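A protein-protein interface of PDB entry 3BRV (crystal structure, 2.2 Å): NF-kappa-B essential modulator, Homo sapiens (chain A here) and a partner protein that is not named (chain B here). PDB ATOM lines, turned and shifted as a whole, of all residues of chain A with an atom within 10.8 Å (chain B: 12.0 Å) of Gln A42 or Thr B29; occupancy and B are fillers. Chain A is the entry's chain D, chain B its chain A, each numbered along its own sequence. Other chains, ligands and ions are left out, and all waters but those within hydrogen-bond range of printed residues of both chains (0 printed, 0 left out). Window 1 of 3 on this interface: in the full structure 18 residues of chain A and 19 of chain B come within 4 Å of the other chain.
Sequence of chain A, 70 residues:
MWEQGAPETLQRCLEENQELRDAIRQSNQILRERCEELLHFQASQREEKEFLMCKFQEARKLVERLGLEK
Printed residues of chain B within 4 Å of Cys A35: Leu B18, Leu B21 and Leu B22.
Of chain B, only Leu B22, Ala B25 and Ile B26 come within 4 Å of Leu A38.
No residue of chain B comes within 4 Å of His A40.
Of the printed residues of chain B, Phe A41 touches Thr B29.
Gln A42 touches just these residues of chain B: Ala B25 (3.2 Å), Asp B28 (3.9 Å) and Thr B29 (3.2 Å).
Ser A44 touches none of the printed residues of chain B.
No residue of chain B comes within 4 Å of Arg A46.
Of the printed residues of chain B, Lys A49 touches Glu B32, Gln B35 and Phe B37.
Cys B19 touches none of the printed residues of chain A.
Printed residues of chain A within 4 Å of Leu B22: Cys A35 and Leu A38.
Ala B25 touches two residues of chain A.
No residue of chain A comes within 4 Å of Gln B27.
Of chain A, only Phe A41, Gln A42 and Gln A45 come within 4 Å of Thr B29.
No residue of chain A comes within 4 Å of Arg B31.
Printed residues of chain A within 4 Å of Gln B35: Lys A49 (2.7 Å).
Ser B36 touches none of the printed residues of chain A.
The nearest printed residue of chain B that does not touch Cys A35 is Ala B25 (4.8 Å).
The side-chain hydroxyl (OG1) of Thr B29 lies within hydrogen-bond range of the backbone carbonyl oxygen (O) of Ala B25.
Of the 20 printed residues of chain B, 11 touch a printed residue of chain A.
Printed residues of chain B that touch a printed residue of chain A: Leu B18, Leu B21, Leu B22, Ala B25, Ile B26, Asp B28, Thr B29, Glu B32, Gln B33, Gln B35 and Phe B37.
Among the printed residues, no Asp or Glu carboxylate lies within 4 Å of a Lys or Arg side-chain nitrogen of the other chain.
The side-chain amino group (NZ) of Lys A49 is in hydrogen-bond range of the backbone carbonyl oxygen (O) of Glu B32 (2.8 Å).
The side-chain hydroxyl of Thr B29 sits at hydrogen-bond distance from the side-chain amide nitrogen of Gln A42, at 3.2 Å.
The side-chain sulfur (SG) of Cys A35 lies within hydrogen-bond range of the backbone NH (N) of Leu B22, at 3.5 Å.
O of Gln B35 sits at hydrogen-bond distance from NZ of Lys A49 (2.7 Å).
O of Ala B25 is in hydrogen-bond range of NE2 of Gln A42 (3.2 Å).
Among the printed residues, pairs that only touch across the chains: Cys A35 with Leu B18 (3.96 Å), Cys A35 with Leu B21 (3.9 Å), Leu A38 with Leu B22 (3.6 Å), Leu A38 with Ala B25 (3.8 Å), Leu A38 with Ile B26 (3.8 Å), Phe A41 with Thr B29 (3.7 Å), Gln A42 with Asp B28 (3.9 Å), Gln A45 with Thr B29 (3.6 Å), Gln A45 with Gln B33 (3.0 Å) and Lys A49 with Phe B37 (3.7 Å).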
ATOM      1  N   ARG A  34      -1.731 -19.156 -32.462  1.00  0.00           N
ATOM      2  CA  ARG A  34      -1.413 -17.866 -32.948  1.00  0.00           C
ATOM      3  C   ARG A  34      -1.979 -16.768 -32.130  1.00  0.00           C
ATOM      4  O   ARG A  34      -1.314 -15.806 -31.919  1.00  0.00           O
ATOM      5  CB  ARG A  34      -2.031 -17.712 -34.338  1.00  0.00           C
ATOM      6  CG  ARG A  34      -1.122 -17.762 -35.486  1.00  0.00           C
ATOM      7  CD  ARG A  34      -0.370 -19.033 -35.596  1.00  0.00           C
ATOM      8  NE  ARG A  34       0.795 -19.251 -34.683  1.00  0.00           N
ATOM      9  CZ  ARG A  34       1.389 -20.470 -34.650  1.00  0.00           C
ATOM     10  NH1 ARG A  34       0.924 -21.454 -35.377  1.00  0.00           N
ATOM     11  NH2 ARG A  34       2.379 -20.769 -33.867  1.00  0.00           N
ATOM     12  N   CYS A  35      -3.228 -16.895 -31.708  1.00  0.00           N
ATOM     13  CA  CYS A  35      -3.861 -15.886 -30.803  1.00  0.00           C
ATOM     14  C   CYS A  35      -3.124 -15.787 -29.488  1.00  0.00           C
ATOM     15  O   CYS A  35      -2.885 -14.685 -28.996  1.00  0.00           O
ATOM     16  CB  CYS A  35      -5.325 -16.129 -30.528  1.00  0.00           C
ATOM     17  SG  CYS A  35      -6.443 -15.924 -31.942  1.00  0.00           S
ATOM     18  N   GLU A  36      -2.704 -16.922 -28.957  1.00  0.00           N
ATOM     19  CA  GLU A  36      -1.953 -16.898 -27.693  1.00  0.00           C
ATOM     20  C   GLU A  36      -0.582 -16.179 -27.819  1.00  0.00           C
ATOM     21  O   GLU A  36      -0.157 -15.513 -26.874  1.00  0.00           O
ATOM     22  CB  GLU A  36      -1.752 -18.276 -27.186  1.00  0.00           C
ATOM     23  CG  GLU A  36      -2.982 -19.104 -27.306  1.00  0.00           C
ATOM     24  CD  GLU A  36      -2.891 -20.358 -26.448  1.00  0.00           C
ATOM     25  OE1 GLU A  36      -3.875 -21.174 -26.410  1.00  0.00           O
ATOM     26  OE2 GLU A  36      -1.807 -20.475 -25.804  1.00  0.00           O
ATOM     27  N   GLU A  37       0.117 -16.410 -28.945  1.00  0.00           N
ATOM     28  CA  GLU A  37       1.414 -15.776 -29.176  1.00  0.00           C
ATOM     29  C   GLU A  37       1.243 -14.291 -29.211  1.00  0.00           C
ATOM     30  O   GLU A  37       2.059 -13.574 -28.700  1.00  0.00           O
ATOM     31  CB  GLU A  37       2.058 -16.225 -30.504  1.00  0.00           C
ATOM     32  CG  GLU A  37       2.508 -17.747 -30.513  1.00  0.00           C
ATOM     33  CD  GLU A  37       2.712 -18.318 -31.938  1.00  0.00           C
ATOM     34  OE1 GLU A  37       2.278 -17.692 -32.922  1.00  0.00           O
ATOM     35  OE2 GLU A  37       3.272 -19.416 -32.102  1.00  0.00           O
ATOM     36  N   LEU A  38       0.192 -13.840 -29.857  1.00  0.00           N
ATOM     37  CA  LEU A  38      -0.143 -12.401 -29.918  1.00  0.00           C
ATOM     38  C   LEU A  38      -0.499 -11.820 -28.549  1.00  0.00           C
ATOM     39  O   LEU A  38      -0.179 -10.656 -28.243  1.00  0.00           O
ATOM     40  CB  LEU A  38      -1.353 -12.202 -30.779  1.00  0.00           C
ATOM     41  CG  LEU A  38      -1.259 -11.717 -32.254  1.00  0.00           C
ATOM     42  CD1 LEU A  38       0.158 -11.471 -32.993  1.00  0.00           C
ATOM     43  CD2 LEU A  38      -2.392 -12.245 -33.204  1.00  0.00           C
ATOM     44  N   LEU A  39      -1.160 -12.597 -27.712  1.00  0.00           N
ATOM     45  CA  LEU A  39      -1.380 -12.132 -26.386  1.00  0.00           C
ATOM     46  C   LEU A  39      -0.057 -11.960 -25.665  1.00  0.00           C
ATOM     47  O   LEU A  39       0.137 -10.960 -24.919  1.00  0.00           O
ATOM     48  CB  LEU A  39      -2.357 -13.037 -25.589  1.00  0.00           C
ATOM     49  CG  LEU A  39      -3.749 -13.139 -26.229  1.00  0.00           C
ATOM     50  CD1 LEU A  39      -4.602 -14.102 -25.490  1.00  0.00           C
ATOM     51  CD2 LEU A  39      -4.512 -11.734 -26.398  1.00  0.00           C
ATOM     52  N   HIS A  40       0.828 -12.948 -25.837  1.00  0.00           N
ATOM     53  CA  HIS A  40       2.165 -12.906 -25.211  1.00  0.00           C
ATOM     54  C   HIS A  40       2.918 -11.711 -25.788  1.00  0.00           C
ATOM     55  O   HIS A  40       3.543 -10.931 -25.050  1.00  0.00           O
ATOM     56  CB  HIS A  40       2.911 -14.239 -25.451  1.00  0.00           C
ATOM     57  CG  HIS A  40       4.335 -14.257 -24.930  1.00  0.00           C
ATOM     58  ND1 HIS A  40       4.645 -14.312 -23.588  1.00  0.00           N
ATOM     59  CD2 HIS A  40       5.526 -14.250 -25.584  1.00  0.00           C
ATOM     60  CE1 HIS A  40       5.958 -14.308 -23.439  1.00  0.00           C
ATOM     61  NE2 HIS A  40       6.512 -14.309 -24.637  1.00  0.00           N
ATOM     62  N   PHE A  41       2.880 -11.558 -27.111  1.00  0.00           N
ATOM     63  CA  PHE A  41       3.564 -10.455 -27.715  1.00  0.00           C
ATOM     64  C   PHE A  41       3.043  -9.078 -27.084  1.00  0.00           C
ATOM     65  O   PHE A  41       3.811  -8.169 -26.779  1.00  0.00           O
ATOM     66  CB  PHE A  41       3.386 -10.506 -29.230  1.00  0.00           C
ATOM     67  CG  PHE A  41       4.014  -9.336 -29.906  1.00  0.00           C
ATOM     68  CD1 PHE A  41       5.418  -9.297 -30.115  1.00  0.00           C
ATOM     69  CD2 PHE A  41       3.238  -8.182 -30.192  1.00  0.00           C
ATOM     70  CE1 PHE A  41       5.995  -8.183 -30.635  1.00  0.00           C
ATOM     71  CE2 PHE A  41       3.847  -7.048 -30.731  1.00  0.00           C
ATOM     72  CZ  PHE A  41       5.203  -7.030 -30.945  1.00  0.00           C
ATOM     73  N   GLN A  42       1.735  -8.933 -26.892  1.00  0.00           N
ATOM     74  CA  GLN A  42       1.208  -7.751 -26.205  1.00  0.00           C
ATOM     75  C   GLN A  42       1.752  -7.577 -24.779  1.00  0.00           C
ATOM     76  O   GLN A  42       2.063  -6.420 -24.383  1.00  0.00           O
ATOM     77  CB  GLN A  42      -0.303  -7.823 -26.109  1.00  0.00           C
ATOM     78  CG  GLN A  42      -1.019  -7.499 -27.411  1.00  0.00           C
ATOM     79  CD  GLN A  42      -2.507  -7.971 -27.393  1.00  0.00           C
ATOM     80  OE1 GLN A  42      -3.181  -7.939 -26.337  1.00  0.00           O
ATOM     81  NE2 GLN A  42      -3.004  -8.406 -28.542  1.00  0.00           N
ATOM     82  N   ALA A  43       1.783  -8.658 -23.970  1.00  0.00           N
ATOM     83  CA  ALA A  43       2.513  -8.552 -22.696  1.00  0.00           C
ATOM     84  C   ALA A  43       4.036  -8.106 -22.818  1.00  0.00           C
ATOM     85  O   ALA A  43       4.516  -7.323 -21.980  1.00  0.00           O
ATOM     86  CB  ALA A  43       2.347  -9.779 -21.887  1.00  0.00           C
ATOM     87  N   SER A  44       4.777  -8.519 -23.864  1.00  0.00           N
ATOM     88  CA  SER A  44       6.164  -8.083 -23.909  1.00  0.00           C
ATOM     89  C   SER A  44       6.306  -6.671 -24.440  1.00  0.00           C
ATOM     90  O   SER A  44       7.260  -6.026 -24.052  1.00  0.00           O
ATOM     91  CB  SER A  44       7.074  -8.971 -24.716  1.00  0.00           C
ATOM     92  OG  SER A  44       6.412 -10.121 -24.802  1.00  0.00           O
ATOM     93  N   GLN A  45       5.439  -6.264 -25.381  1.00  0.00           N
ATOM     94  CA  GLN A  45       5.352  -4.889 -25.872  1.00  0.00           C
ATOM     95  C   GLN A  45       5.100  -3.917 -24.672  1.00  0.00           C
ATOM     96  O   GLN A  45       5.784  -2.927 -24.521  1.00  0.00           O
ATOM     97  CB  GLN A  45       4.285  -4.747 -26.983  1.00  0.00           C
ATOM     98  CG  GLN A  45       4.315  -3.320 -27.617  1.00  0.00           C
ATOM     99  CD  GLN A  45       3.706  -3.172 -29.054  1.00  0.00           C
ATOM    100  OE1 GLN A  45       2.531  -3.496 -29.312  1.00  0.00           O
ATOM    101  NE2 GLN A  45       4.508  -2.603 -29.963  1.00  0.00           N
ATOM    102  N   ARG A  46       4.148  -4.263 -23.822  1.00  0.00           N
ATOM    103  CA  ARG A  46       3.849  -3.544 -22.636  1.00  0.00           C
ATOM    104  C   ARG A  46       5.019  -3.496 -21.645  1.00  0.00           C
ATOM    105  O   ARG A  46       5.319  -2.448 -21.158  1.00  0.00           O
ATOM    106  CB  ARG A  46       2.549  -4.097 -22.020  1.00  0.00           C
ATOM    107  CG  ARG A  46       1.945  -3.260 -20.933  1.00  0.00           C
ATOM    108  CD  ARG A  46       0.750  -3.994 -20.229  1.00  0.00           C
ATOM    109  NE  ARG A  46      -0.083  -4.751 -21.207  1.00  0.00           N
ATOM    110  CZ  ARG A  46      -0.232  -6.095 -21.246  1.00  0.00           C
ATOM    111  NH1 ARG A  46       0.395  -6.901 -20.363  1.00  0.00           N
ATOM    112  NH2 ARG A  46      -1.031  -6.642 -22.162  1.00  0.00           N
ATOM    113  N   GLU A  47       5.717  -4.600 -21.399  1.00  0.00           N
ATOM    114  CA  GLU A  47       6.913  -4.508 -20.551  1.00  0.00           C
ATOM    115  C   GLU A  47       8.000  -3.650 -21.183  1.00  0.00           C
ATOM    116  O   GLU A  47       8.691  -2.973 -20.455  1.00  0.00           O
ATOM    117  CB  GLU A  47       7.491  -5.885 -20.098  1.00  0.00           C
ATOM    118  N   GLU A  48       8.177  -3.705 -22.505  1.00  0.00           N
ATOM    119  CA  GLU A  48       9.204  -2.896 -23.176  1.00  0.00           C
ATOM    120  C   GLU A  48       8.919  -1.359 -23.084  1.00  0.00           C
ATOM    121  O   GLU A  48       9.854  -0.578 -22.900  1.00  0.00           O
ATOM    122  CB  GLU A  48       9.407  -3.297 -24.638  1.00  0.00           C
ATOM    123  CG  GLU A  48      10.559  -2.562 -25.346  1.00  0.00           C
ATOM    124  CD  GLU A  48      11.953  -3.195 -25.080  1.00  0.00           C
ATOM    125  OE1 GLU A  48      12.906  -2.853 -25.841  1.00  0.00           O
ATOM    126  OE2 GLU A  48      12.082  -4.059 -24.134  1.00  0.00           O
ATOM    127  N   LYS A  49       7.676  -0.937 -23.285  1.00  0.00           N
ATOM    128  CA  LYS A  49       7.351   0.478 -23.190  1.00  0.00           C
ATOM    129  C   LYS A  49       7.529   1.050 -21.747  1.00  0.00           C
ATOM    130  O   LYS A  49       7.894   2.219 -21.557  1.00  0.00           O
ATOM    131  CB  LYS A  49       5.903   0.618 -23.549  1.00  0.00           C
ATOM    132  CG  LYS A  49       5.627   0.990 -24.980  1.00  0.00           C
ATOM    133  CD  LYS A  49       4.320   1.788 -25.078  1.00  0.00           C
ATOM    134  CE  LYS A  49       4.296   2.588 -26.368  1.00  0.00           C
ATOM    135  NZ  LYS A  49       3.067   2.147 -27.120  1.00  0.00           N
ATOM    136  N   GLU A  50       7.153   0.264 -20.753  1.00  0.00           N
ATOM    137  CA  GLU A  50       7.252   0.633 -19.338  1.00  0.00           C
ATOM    138  C   GLU A  50       8.682   0.869 -19.004  1.00  0.00           C
ATOM    139  O   GLU A  50       9.001   1.853 -18.484  1.00  0.00           O
ATOM    140  CB  GLU A  50       6.607  -0.444 -18.443  1.00  0.00           C
ATOM    141  N   LEU B  18     -12.572 -17.982 -34.007  1.00  0.00           N
ATOM    142  CA  LEU B  18     -11.100 -17.822 -33.897  1.00  0.00           C
ATOM    143  C   LEU B  18     -10.502 -16.720 -34.780  1.00  0.00           C
ATOM    144  O   LEU B  18      -9.578 -16.041 -34.363  1.00  0.00           O
ATOM    145  CB  LEU B  18     -10.358 -19.155 -34.163  1.00  0.00           C
ATOM    146  CG  LEU B  18     -10.748 -20.157 -33.049  1.00  0.00           C
ATOM    147  CD1 LEU B  18     -10.322 -21.533 -33.443  1.00  0.00           C
ATOM    148  CD2 LEU B  18     -10.152 -19.760 -31.694  1.00  0.00           C
ATOM    149  N   CYS B  19     -11.081 -16.554 -35.957  1.00  0.00           N
ATOM    150  CA  CYS B  19     -10.762 -15.459 -36.869  1.00  0.00           C
ATOM    151  C   CYS B  19     -11.124 -14.106 -36.308  1.00  0.00           C
ATOM    152  O   CYS B  19     -10.439 -13.125 -36.606  1.00  0.00           O
ATOM    153  CB  CYS B  19     -11.418 -15.657 -38.279  1.00  0.00           C
ATOM    154  SG  CYS B  19     -10.621 -17.033 -39.271  1.00  0.00           S
ATOM    155  N   THR B  20     -12.219 -14.051 -35.567  1.00  0.00           N
ATOM    156  CA  THR B  20     -12.673 -12.827 -35.005  1.00  0.00           C
ATOM    157  C   THR B  20     -11.675 -12.413 -33.898  1.00  0.00           C
ATOM    158  O   THR B  20     -11.175 -11.265 -33.938  1.00  0.00           O
ATOM    159  CB  THR B  20     -14.108 -12.945 -34.488  1.00  0.00           C
ATOM    160  OG1 THR B  20     -14.984 -13.243 -35.572  1.00  0.00           O
ATOM    161  CG2 THR B  20     -14.591 -11.630 -33.834  1.00  0.00           C
ATOM    162  N   LEU B  21     -11.378 -13.363 -32.975  1.00  0.00           N
ATOM    163  CA  LEU B  21     -10.257 -13.286 -31.978  1.00  0.00           C
ATOM    164  C   LEU B  21      -8.894 -12.955 -32.580  1.00  0.00           C
ATOM    165  O   LEU B  21      -8.247 -12.045 -32.093  1.00  0.00           O
ATOM    166  CB  LEU B  21     -10.162 -14.526 -31.047  1.00  0.00           C
ATOM    167  CG  LEU B  21     -11.389 -14.680 -30.146  1.00  0.00           C
ATOM    168  CD1 LEU B  21     -11.529 -16.041 -29.537  1.00  0.00           C
ATOM    169  CD2 LEU B  21     -11.422 -13.647 -29.086  1.00  0.00           C
ATOM    170  N   LEU B  22      -8.440 -13.650 -33.626  1.00  0.00           N
ATOM    171  CA  LEU B  22      -7.226 -13.233 -34.318  1.00  0.00           C
ATOM    172  C   LEU B  22      -7.363 -11.788 -34.844  1.00  0.00           C
ATOM    173  O   LEU B  22      -6.463 -10.968 -34.697  1.00  0.00           O
ATOM    174  CB  LEU B  22      -6.899 -14.182 -35.452  1.00  0.00           C
ATOM    175  CG  LEU B  22      -5.631 -13.833 -36.259  1.00  0.00           C
ATOM    176  CD1 LEU B  22      -4.386 -14.239 -35.422  1.00  0.00           C
ATOM    177  CD2 LEU B  22      -5.540 -14.539 -37.679  1.00  0.00           C
ATOM    178  N   GLU B  23      -8.447 -11.472 -35.491  1.00  0.00           N
ATOM    179  CA  GLU B  23      -8.667 -10.093 -35.896  1.00  0.00           C
ATOM    180  C   GLU B  23      -8.484  -9.098 -34.771  1.00  0.00           C
ATOM    181  O   GLU B  23      -7.763  -8.096 -34.943  1.00  0.00           O
ATOM    182  CB  GLU B  23      -9.997  -9.904 -36.638  1.00  0.00           C
ATOM    183  CG  GLU B  23      -9.797 -10.371 -38.106  1.00  0.00           C
ATOM    184  CD  GLU B  23     -10.980 -10.130 -39.018  1.00  0.00           C
ATOM    185  OE1 GLU B  23     -10.818  -9.313 -40.019  1.00  0.00           O
ATOM    186  OE2 GLU B  23     -12.049 -10.756 -38.718  1.00  0.00           O
ATOM    187  N   ASN B  24      -9.140  -9.355 -33.647  1.00  0.00           N
ATOM    188  CA  ASN B  24      -9.168  -8.421 -32.493  1.00  0.00           C
ATOM    189  C   ASN B  24      -7.775  -8.246 -31.875  1.00  0.00           C
ATOM    190  O   ASN B  24      -7.375  -7.126 -31.469  1.00  0.00           O
ATOM    191  CB  ASN B  24     -10.056  -8.984 -31.423  1.00  0.00           C
ATOM    192  CG  ASN B  24     -11.528  -8.885 -31.765  1.00  0.00           C
ATOM    193  OD1 ASN B  24     -12.406  -9.405 -31.022  1.00  0.00           O
ATOM    194  ND2 ASN B  24     -11.835  -8.176 -32.858  1.00  0.00           N
ATOM    195  N   ALA B  25      -7.080  -9.392 -31.772  1.00  0.00           N
ATOM    196  CA  ALA B  25      -5.774  -9.524 -31.155  1.00  0.00           C
ATOM    197  C   ALA B  25      -4.846  -8.711 -32.009  1.00  0.00           C
ATOM    198  O   ALA B  25      -4.079  -7.981 -31.474  1.00  0.00           O
ATOM    199  CB  ALA B  25      -5.308 -11.043 -31.065  1.00  0.00           C
ATOM    200  N   ILE B  26      -4.927  -8.805 -33.336  1.00  0.00           N
ATOM    201  CA  ILE B  26      -3.999  -8.032 -34.201  1.00  0.00           C
ATOM    202  C   ILE B  26      -4.290  -6.543 -34.087  1.00  0.00           C
ATOM    203  O   ILE B  26      -3.341  -5.701 -34.125  1.00  0.00           O
ATOM    204  CB  ILE B  26      -4.059  -8.451 -35.707  1.00  0.00           C
ATOM    205  CG1 ILE B  26      -3.832  -9.966 -35.926  1.00  0.00           C
ATOM    206  CG2 ILE B  26      -3.246  -7.500 -36.647  1.00  0.00           C
ATOM    207  CD1 ILE B  26      -2.580 -10.361 -36.464  1.00  0.00           C
ATOM    208  N   GLN B  27      -5.582  -6.208 -34.012  1.00  0.00           N
ATOM    209  CA  GLN B  27      -6.025  -4.815 -33.946  1.00  0.00           C
ATOM    210  C   GLN B  27      -5.517  -4.132 -32.679  1.00  0.00           C
ATOM    211  O   GLN B  27      -5.040  -3.025 -32.739  1.00  0.00           O
ATOM    212  CB  GLN B  27      -7.572  -4.648 -34.062  1.00  0.00           C
ATOM    213  N   ASP B  28      -5.675  -4.791 -31.539  1.00  0.00           N
ATOM    214  CA  ASP B  28      -5.178  -4.318 -30.268  1.00  0.00           C
ATOM    215  C   ASP B  28      -3.699  -4.014 -30.310  1.00  0.00           C
ATOM    216  O   ASP B  28      -3.269  -2.953 -29.846  1.00  0.00           O
ATOM    217  CB  ASP B  28      -5.334  -5.413 -29.235  1.00  0.00           C
ATOM    218  CG  ASP B  28      -6.507  -5.217 -28.351  1.00  0.00           C
ATOM    219  OD1 ASP B  28      -6.611  -4.109 -27.695  1.00  0.00           O
ATOM    220  OD2 ASP B  28      -7.301  -6.207 -28.268  1.00  0.00           O
ATOM    221  N   THR B  29      -2.941  -4.962 -30.838  1.00  0.00           N
ATOM    222  CA  THR B  29      -1.514  -4.818 -30.988  1.00  0.00           C
ATOM    223  C   THR B  29      -1.160  -3.578 -31.785  1.00  0.00           C
ATOM    224  O   THR B  29      -0.357  -2.782 -31.309  1.00  0.00           O
ATOM    225  CB  THR B  29      -0.903  -6.054 -31.666  1.00  0.00           C
ATOM    226  OG1 THR B  29      -1.106  -7.169 -30.823  1.00  0.00           O
ATOM    227  CG2 THR B  29       0.536  -5.888 -31.873  1.00  0.00           C
ATOM    228  N   VAL B  30      -1.732  -3.439 -32.980  1.00  0.00           N
ATOM    229  CA  VAL B  30      -1.495  -2.275 -33.851  1.00  0.00           C
ATOM    230  C   VAL B  30      -2.382  -1.131 -33.359  1.00  0.00           C
ATOM    231  O   VAL B  30      -3.233  -0.678 -34.112  1.00  0.00           O
ATOM    232  CB  VAL B  30      -2.059  -2.434 -35.297  1.00  0.00           C
ATOM    233  CG1 VAL B  30      -1.682  -1.156 -36.153  1.00  0.00           C
ATOM    234  CG2 VAL B  30      -1.729  -3.761 -35.986  1.00  0.00           C
ATOM    235  N   ARG B  31      -2.307  -0.709 -32.120  1.00  0.00           N
ATOM    236  CA  ARG B  31      -3.171   0.392 -31.622  1.00  0.00           C
ATOM    237  C   ARG B  31      -2.350   0.769 -30.420  1.00  0.00           C
ATOM    238  O   ARG B  31      -1.951   1.911 -30.252  1.00  0.00           O
ATOM    239  CB  ARG B  31      -4.590  -0.066 -31.224  1.00  0.00           C
ATOM    240  N   GLU B  32      -2.010  -0.240 -29.621  1.00  0.00           N
ATOM    241  CA  GLU B  32      -1.013  -0.060 -28.568  1.00  0.00           C
ATOM    242  C   GLU B  32       0.311   0.491 -29.143  1.00  0.00           C
ATOM    243  O   GLU B  32       0.780   1.505 -28.682  1.00  0.00           O
ATOM    244  CB  GLU B  32      -0.836  -1.364 -27.764  1.00  0.00           C
ATOM    245  N   GLN B  33       0.854  -0.110 -30.210  1.00  0.00           N
ATOM    246  CA  GLN B  33       2.172   0.300 -30.725  1.00  0.00           C
ATOM    247  C   GLN B  33       2.096   1.645 -31.459  1.00  0.00           C
ATOM    248  O   GLN B  33       3.146   2.306 -31.758  1.00  0.00           O
ATOM    249  CB  GLN B  33       2.811  -0.791 -31.575  1.00  0.00           C
ATOM    250  CG  GLN B  33       4.295  -0.501 -32.155  1.00  0.00           C
ATOM    251  CD  GLN B  33       4.378   0.352 -33.451  1.00  0.00           C
ATOM    252  OE1 GLN B  33       5.474   0.764 -33.863  1.00  0.00           O
ATOM    253  NE2 GLN B  33       3.245   0.600 -34.092  1.00  0.00           N
ATOM    254  N   ASP B  34       0.856   2.074 -31.700  1.00  0.00           N
ATOM    255  CA  ASP B  34       0.579   3.446 -32.177  1.00  0.00           C
ATOM    256  C   ASP B  34       0.504   4.513 -31.131  1.00  0.00           C
ATOM    257  O   ASP B  34       0.303   5.654 -31.455  1.00  0.00           O
ATOM    258  CB  ASP B  34      -0.663   3.483 -33.020  1.00  0.00           C
ATOM    259  CG  ASP B  34      -0.332   3.445 -34.481  1.00  0.00           C
ATOM    260  OD1 ASP B  34       0.268   4.452 -34.994  1.00  0.00           O
ATOM    261  OD2 ASP B  34      -0.659   2.409 -35.099  1.00  0.00           O
ATOM    262  N   GLN B  35       0.630   4.154 -29.862  1.00  0.00           N
ATOM    263  CA  GLN B  35       0.909   5.176 -28.874  1.00  0.00           C
ATOM    264  C   GLN B  35       2.457   5.330 -28.938  1.00  0.00           C
ATOM    265  O   GLN B  35       3.193   4.478 -28.448  1.00  0.00           O
ATOM    266  CB  GLN B  35       0.340   4.769 -27.503  1.00  0.00           C
ATOM    267  CG  GLN B  35      -1.179   4.521 -27.541  1.00  0.00           C
ATOM    268  CD  GLN B  35      -2.005   5.776 -27.884  1.00  0.00           C
ATOM    269  OE1 GLN B  35      -1.960   6.790 -27.158  1.00  0.00           O
ATOM    270  NE2 GLN B  35      -2.784   5.704 -28.982  1.00  0.00           N
ATOM    271  N   SER B  36       2.917   6.369 -29.634  1.00  0.00           N
ATOM    272  CA  SER B  36       4.362   6.494 -29.979  1.00  0.00           C
ATOM    273  C   SER B  36       5.143   7.444 -29.071  1.00  0.00           C
ATOM    274  O   SER B  36       4.605   8.472 -28.527  1.00  0.00           O
ATOM    275  CB  SER B  36       4.531   6.810 -31.478  1.00  0.00           C
ATOM    276  OG  SER B  36       5.813   7.362 -31.782  1.00  0.00           O
ATOM    277  N   PHE B  37       6.424   7.135 -28.922  1.00  0.00           N
ATOM    278  CA  PHE B  37       7.336   7.974 -28.157  1.00  0.00           C
ATOM    279  C   PHE B  37       7.636   9.294 -28.834  1.00  0.00           C
ATOM    280  O   PHE B  37       8.140  10.227 -28.207  1.00  0.00           O
ATOM    281  CB  PHE B  37       8.606   7.193 -27.865  1.00  0.00           C
ATOM    282  CG  PHE B  37       8.466   6.168 -26.722  1.00  0.00           C
ATOM    283  CD1 PHE B  37       7.980   4.909 -26.943  1.00  0.00           C
ATOM    284  CD2 PHE B  37       8.883   6.488 -25.421  1.00  0.00           C
ATOM    285  CE1 PHE B  37       7.869   3.962 -25.872  1.00  0.00           C
ATOM    286  CE2 PHE B  37       8.795   5.554 -24.351  1.00  0.00           C
ATOM    287  CZ  PHE B  37       8.273   4.308 -24.587  1.00  0.00           C
